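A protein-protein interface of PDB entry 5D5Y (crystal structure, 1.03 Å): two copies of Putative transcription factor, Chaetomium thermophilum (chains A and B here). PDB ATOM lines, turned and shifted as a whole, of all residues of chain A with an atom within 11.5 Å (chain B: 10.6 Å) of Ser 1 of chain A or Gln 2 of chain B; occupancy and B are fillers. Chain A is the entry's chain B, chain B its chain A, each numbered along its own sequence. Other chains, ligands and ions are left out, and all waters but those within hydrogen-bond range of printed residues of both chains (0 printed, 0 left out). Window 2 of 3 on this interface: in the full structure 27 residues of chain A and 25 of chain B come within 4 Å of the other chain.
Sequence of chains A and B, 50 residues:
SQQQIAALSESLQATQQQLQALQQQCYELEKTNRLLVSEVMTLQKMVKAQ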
ATOM      1  N   SER A   1      25.577  -3.189 -17.935  1.00  0.00           N
ATOM      2  CA  SER A   1      24.350  -2.435 -17.477  1.00  0.00           C
ATOM      3  C   SER A   1      24.264  -2.304 -15.961  1.00  0.00           C
ATOM      4  O   SER A   1      24.421  -1.213 -15.385  1.00  0.00           O
ATOM      5  CB  SER A   1      23.087  -3.127 -17.968  1.00  0.00           C
ATOM      6  OG  SER A   1      22.023  -2.210 -18.184  1.00  0.00           O
ATOM      7  N   GLN A   2      24.043  -3.439 -15.307  1.00  0.00           N
ATOM      8  CA  GLN A   2      23.482  -3.438 -13.962  1.00  0.00           C
ATOM      9  C   GLN A   2      24.433  -3.163 -12.803  1.00  0.00           C
ATOM     10  O   GLN A   2      23.994  -3.049 -11.649  1.00  0.00           O
ATOM     11  CB  GLN A   2      22.788  -4.743 -13.743  1.00  0.00           C
ATOM     12  CG  GLN A   2      21.391  -4.784 -14.264  1.00  0.00           C
ATOM     13  CD  GLN A   2      20.790  -6.085 -13.832  1.00  0.00           C
ATOM     14  OE1 GLN A   2      19.554  -6.280 -13.796  1.00  0.00           O
ATOM     15  NE2 GLN A   2      21.645  -6.970 -13.415  1.00  0.00           N
ATOM     16  N   GLN A   3      25.721  -3.071 -13.079  1.00  0.00           N
ATOM     17  CA  GLN A   3      26.635  -2.679 -12.033  1.00  0.00           C
ATOM     18  C   GLN A   3      26.223  -1.234 -11.689  1.00  0.00           C
ATOM     19  O   GLN A   3      25.782  -0.878 -10.539  1.00  0.00           O
ATOM     20  CB  GLN A   3      28.091  -2.775 -12.521  1.00  0.00           C
ATOM     21  N   GLN A   4      26.311  -0.417 -12.734  1.00  0.00           N
ATOM     22  CA  GLN A   4      26.127   0.985 -12.568  1.00  0.00           C
ATOM     23  C   GLN A   4      24.675   1.288 -12.339  1.00  0.00           C
ATOM     24  O   GLN A   4      24.418   2.067 -11.431  1.00  0.00           O
ATOM     25  CB  GLN A   4      26.709   1.793 -13.719  1.00  0.00           C
ATOM     26  CG  GLN A   4      28.206   1.711 -13.826  1.00  0.00           C
ATOM     27  CD  GLN A   4      28.950   2.146 -12.588  1.00  0.00           C
ATOM     28  OE1 GLN A   4      28.419   2.874 -11.718  1.00  0.00           O
ATOM     29  NE2 GLN A   4      30.191   1.661 -12.464  1.00  0.00           N
ATOM     30  N   ILE A   5      23.715   0.671 -13.037  1.00  0.00           N
ATOM     31  CA  ILE A   5      22.303   0.958 -12.726  1.00  0.00           C
ATOM     32  C   ILE A   5      21.819   0.591 -11.254  1.00  0.00           C
ATOM     33  O   ILE A   5      20.999   1.475 -10.665  1.00  0.00           O
ATOM     34  CB  ILE A   5      21.333   0.270 -13.714  1.00  0.00           C
ATOM     35  CG1 ILE A   5      21.097   1.152 -14.944  1.00  0.00           C
ATOM     36  CG2 ILE A   5      19.991  -0.004 -13.029  1.00  0.00           C
ATOM     37  CD1 ILE A   5      21.905   0.751 -16.142  1.00  0.00           C
ATOM     38  N   ALA A   6      22.660  -0.485 -10.658  1.00  0.00           N
ATOM     39  CA  ALA A   6      22.246  -0.899  -9.301  1.00  0.00           C
ATOM     40  C   ALA A   6      22.784   0.134  -8.273  1.00  0.00           C
ATOM     41  O   ALA A   6      22.104   0.505  -7.254  1.00  0.00           O
ATOM     42  CB  ALA A   6      22.756  -2.320  -8.996  1.00  0.00           C
ATOM     43  N   ALA A   7      24.025   0.588  -8.509  1.00  0.00           N
ATOM     44  CA  ALA A   7      24.614   1.628  -7.662  1.00  0.00           C
ATOM     45  C   ALA A   7      23.838   2.923  -7.884  1.00  0.00           C
ATOM     46  O   ALA A   7      23.572   3.646  -6.956  1.00  0.00           O
ATOM     47  CB  ALA A   7      26.089   1.829  -7.986  1.00  0.00           C
ATOM     48  N   LEU A   8      23.373   3.197  -9.094  1.00  0.00           N
ATOM     49  CA  LEU A   8      22.600   4.440  -9.291  1.00  0.00           C
ATOM     50  C   LEU A   8      21.271   4.328  -8.547  1.00  0.00           C
ATOM     51  O   LEU A   8      20.839   5.269  -7.913  1.00  0.00           O
ATOM     52  CB  LEU A   8      22.371   4.678 -10.769  1.00  0.00           C
ATOM     53  CG  LEU A   8      21.409   5.811 -11.173  1.00  0.00           C
ATOM     54  CD1 LEU A   8      21.778   7.163 -10.578  1.00  0.00           C
ATOM     55  CD2 LEU A   8      21.391   5.875 -12.687  1.00  0.00           C
ATOM     56  N   SER A   9      20.632   3.169  -8.621  1.00  0.00           N
ATOM     57  CA  SER A   9      19.378   2.906  -7.877  1.00  0.00           C
ATOM     58  C   SER A   9      19.540   3.095  -6.343  1.00  0.00           C
ATOM     59  O   SER A   9      18.716   3.701  -5.636  1.00  0.00           O
ATOM     60  CB  SER A   9      18.868   1.522  -8.115  1.00  0.00           C
ATOM     61  OG  SER A   9      17.820   1.171  -7.217  1.00  0.00           O
ATOM     62  N   GLU A  10      20.637   2.573  -5.821  1.00  0.00           N
ATOM     63  CA  GLU A  10      20.984   2.671  -4.427  1.00  0.00           C
ATOM     64  C   GLU A  10      21.191   4.135  -4.095  1.00  0.00           C
ATOM     65  O   GLU A  10      20.773   4.613  -3.005  1.00  0.00           O
ATOM     66  CB  GLU A  10      22.252   1.902  -4.105  1.00  0.00           C
ATOM     67  CG  GLU A  10      22.739   1.954  -2.663  1.00  0.00           C
ATOM     68  CD  GLU A  10      23.893   0.988  -2.398  1.00  0.00           C
ATOM     69  OE1 GLU A  10      24.263   0.228  -3.330  1.00  0.00           O
ATOM     70  OE2 GLU A  10      24.435   1.001  -1.265  1.00  0.00           O
ATOM     71  N   SER B   1      26.887   4.318 -21.761  1.00  0.00           N
ATOM     72  CA  SER B   1      28.133   3.712 -21.201  1.00  0.00           C
ATOM     73  C   SER B   1      28.050   3.582 -19.699  1.00  0.00           C
ATOM     74  O   SER B   1      27.165   4.185 -19.030  1.00  0.00           O
ATOM     75  CB  SER B   1      29.356   4.556 -21.523  1.00  0.00           C
ATOM     76  OG  SER B   1      29.302   5.810 -20.948  1.00  0.00           O
ATOM     77  N   GLN B   2      28.967   2.806 -19.138  1.00  0.00           N
ATOM     78  CA  GLN B   2      29.047   2.705 -17.681  1.00  0.00           C
ATOM     79  C   GLN B   2      29.531   4.015 -17.065  1.00  0.00           C
ATOM     80  O   GLN B   2      29.077   4.457 -15.967  1.00  0.00           O
ATOM     81  CB  GLN B   2      29.943   1.577 -17.213  1.00  0.00           C
ATOM     82  CG  GLN B   2      29.555   0.219 -17.783  1.00  0.00           C
ATOM     83  CD  GLN B   2      28.114  -0.199 -17.492  1.00  0.00           C
ATOM     84  OE1 GLN B   2      27.361  -0.628 -18.385  1.00  0.00           O
ATOM     85  NE2 GLN B   2      27.744  -0.128 -16.244  1.00  0.00           N
ATOM     86  N   GLN B   3      30.412   4.688 -17.789  1.00  0.00           N
ATOM     87  CA  GLN B   3      30.882   6.012 -17.356  1.00  0.00           C
ATOM     88  C   GLN B   3      29.704   6.984 -17.137  1.00  0.00           C
ATOM     89  O   GLN B   3      29.681   7.778 -16.186  1.00  0.00           O
ATOM     90  CB  GLN B   3      31.824   6.653 -18.370  1.00  0.00           C
ATOM     91  N   GLN B   4      28.712   6.943 -18.017  1.00  0.00           N
ATOM     92  CA  GLN B   4      27.590   7.880 -17.933  1.00  0.00           C
ATOM     93  C   GLN B   4      26.768   7.595 -16.694  1.00  0.00           C
ATOM     94  O   GLN B   4      26.301   8.491 -15.993  1.00  0.00           O
ATOM     95  CB  GLN B   4      26.670   7.749 -19.147  1.00  0.00           C
ATOM     96  CG  GLN B   4      27.269   8.203 -20.463  1.00  0.00           C
ATOM     97  CD  GLN B   4      27.825   9.608 -20.444  1.00  0.00           C
ATOM     98  OE1 GLN B   4      27.289  10.504 -19.774  1.00  0.00           O
ATOM     99  NE2 GLN B   4      28.893   9.823 -21.209  1.00  0.00           N
ATOM    100  N   ILE B   5      26.554   6.316 -16.447  1.00  0.00           N
ATOM    101  CA  ILE B   5      25.776   5.922 -15.273  1.00  0.00           C
ATOM    102  C   ILE B   5      26.505   6.323 -13.970  1.00  0.00           C
ATOM    103  O   ILE B   5      25.880   6.963 -12.981  1.00  0.00           O
ATOM    104  CB  ILE B   5      25.461   4.423 -15.315  1.00  0.00           C
ATOM    105  CG1 ILE B   5      24.718   4.067 -16.596  1.00  0.00           C
ATOM    106  CG2 ILE B   5      24.538   4.102 -14.144  1.00  0.00           C
ATOM    107  CD1 ILE B   5      24.623   2.581 -16.857  1.00  0.00           C
ATOM    108  N   ALA B   6      27.813   6.095 -13.960  1.00  0.00           N
ATOM    109  CA  ALA B   6      28.626   6.472 -12.817  1.00  0.00           C
ATOM    110  C   ALA B   6      28.507   7.982 -12.554  1.00  0.00           C
ATOM    111  O   ALA B   6      28.447   8.422 -11.392  1.00  0.00           O
ATOM    112  CB  ALA B   6      30.084   6.075 -13.015  1.00  0.00           C
ATOM    113  N   ALA B   7      28.463   8.804 -13.599  1.00  0.00           N
ATOM    114  CA  ALA B   7      28.445  10.239 -13.453  1.00  0.00           C
ATOM    115  C   ALA B   7      27.148  10.631 -12.840  1.00  0.00           C
ATOM    116  O   ALA B   7      27.132  11.489 -12.056  1.00  0.00           O
ATOM    117  CB  ALA B   7      28.600  10.900 -14.819  1.00  0.00           C
ATOM    118  N   LEU B   8      26.068   9.969 -13.207  1.00  0.00           N
ATOM    119  CA  LEU B   8      24.774  10.265 -12.630  1.00  0.00           C
ATOM    120  C   LEU B   8      24.697   9.918 -11.130  1.00  0.00           C
ATOM    121  O   LEU B   8      24.141  10.660 -10.329  1.00  0.00           O
ATOM    122  CB  LEU B   8      23.664   9.542 -13.391  1.00  0.00           C
ATOM    123  CG  LEU B   8      23.445   9.953 -14.858  1.00  0.00           C
ATOM    124  CD1 LEU B   8      22.426   9.011 -15.493  1.00  0.00           C
ATOM    125  CD2 LEU B   8      23.018  11.395 -15.065  1.00  0.00           C
ATOM    126  N   SER B   9      25.249   8.751 -10.810  1.00  0.00           N
ATOM    127  CA  SER B   9      25.281   8.310  -9.401  1.00  0.00           C
ATOM    128  C   SER B   9      26.064   9.290  -8.539  1.00  0.00           C
ATOM    129  O   SER B   9      25.580   9.700  -7.466  1.00  0.00           O
ATOM    130  CB  SER B   9      25.864   6.912  -9.350  1.00  0.00           C
ATOM    131  OG  SER B   9      25.829   6.428  -8.045  1.00  0.00           O
ATOM    132  N   GLU B  10      27.224   9.740  -9.015  1.00  0.00           N
ATOM    133  CA  GLU B  10      28.013  10.724  -8.292  1.00  0.00           C
ATOM    134  C   GLU B  10      27.254  12.024  -8.180  1.00  0.00           C
ATOM    135  O   GLU B  10      27.286  12.689  -7.134  1.00  0.00           O
ATOM    136  CB  GLU B  10      29.328  10.993  -8.986  1.00  0.00           C
ATOM    137  CG  GLU B  10      30.317   9.854  -8.857  1.00  0.00           C
ATOM    138  CD  GLU B  10      30.610   9.480  -7.416  1.00  0.00           C
ATOM    139  OE1 GLU B  10      30.991  10.376  -6.626  1.00  0.00           O
ATOM    140  OE2 GLU B  10      30.464   8.283  -7.077  1.00  0.00           O
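The side-chain amide oxygen of Gln 2 of chain B is in hydrogen-bond range of the backbone NH of Ser 1 of chain A, 3.2 Å away.
Among the printed residues, merely in contact across the chains: Gln 4 of chain A with Gln 2 of chain B, Gln 4 of chain A with Ile 5 of chain B, Ile 5 of chain A with Ile 5 of chain B, Ala 7 of chain A with Ser 9 of chain B, Gln 4 of chain A with Ala 6 of chain B, Leu 8 of chain A with Ser 9 of chain B and Leu 8 of chain A with Ile 5 of chain B.
Printed residues of chain B within 4 Å of Ser 1 of chain A: Gln 2 (3.2 Å).
No residue of chain B comes within 4 Å of Gln 3 of chain A.
Gln 4 of chain A touches just these residues of chain B: Gln 2, Ile 5 and Ala 6.
Printed residues of chain B within 4 Å of Ala 7 of chain A: Ser 9 (3.7 Å).
Of the printed residues of chain B, Leu 8 of chain A touches Ile 5 (3.9 Å) and Ser 9 (3.8 Å).
Ser 1 of chain B touches none of the printed residues of chain A.
Gln 2 of chain B touches just these residues of chain A: Ser 1 (3.2 Å) and Gln 4 (3.1 Å).
No residue of chain A comes within 4 Å of Gln 3 of chain B.
Ile 5 of chain B touches just these residues of chain A: Gln 4, Ile 5 and Leu 8.
Leu 8 of chain B touches none of the printed residues of chain A.
Printed residues of chain A within 4 Å of Ser 9 of chain B: Ala 7 and Leu 8.
Glu 10 of chain B touches none of the printed residues of chain A.
Of the 10 printed residues of chain A, 5 touch a printed residue of chain B.
Hydrophobic or aromatic side chains of chain A that line the printed part of chain B: Ile 5 and Leu 8.
Along chain A the printed residues that touch a printed residue of chain B span positions 1 to 8.
Hydrophobic or aromatic side chains of chain B within 4 Å of the printed part of chain A: Ile 5 and Ala 6.
Among the printed residues, 8 pairs touch across the chains.
Among the printed residues, no Asp or Glu carboxylate lies within 4 Å of a Lys or Arg side-chain nitrogen of the other chain.
Gln 4 of chain A touches Ile 5 of chain B, but with the chains exchanged Ile 5 of chain A does not touch Gln 4 of chain B (8.4 Å).
Gln 4 of chain A touches Ala 6 of chain B, but with the chains exchanged Ala 6 of chain A does not touch Gln 4 of chain B (10.9 Å).
Ile 5 of chain A touches its own counterpart, Ile 5 of chain B.
Leu 8 of chain A touches Ile 5 of chain B, but with the chains exchanged Ile 5 of chain A does not touch Leu 8 of chain B (8.0 Å).
Of the 8 pairs that touch across the chains among the printed residues, 1 has its exchanged pair printed and touching as well.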
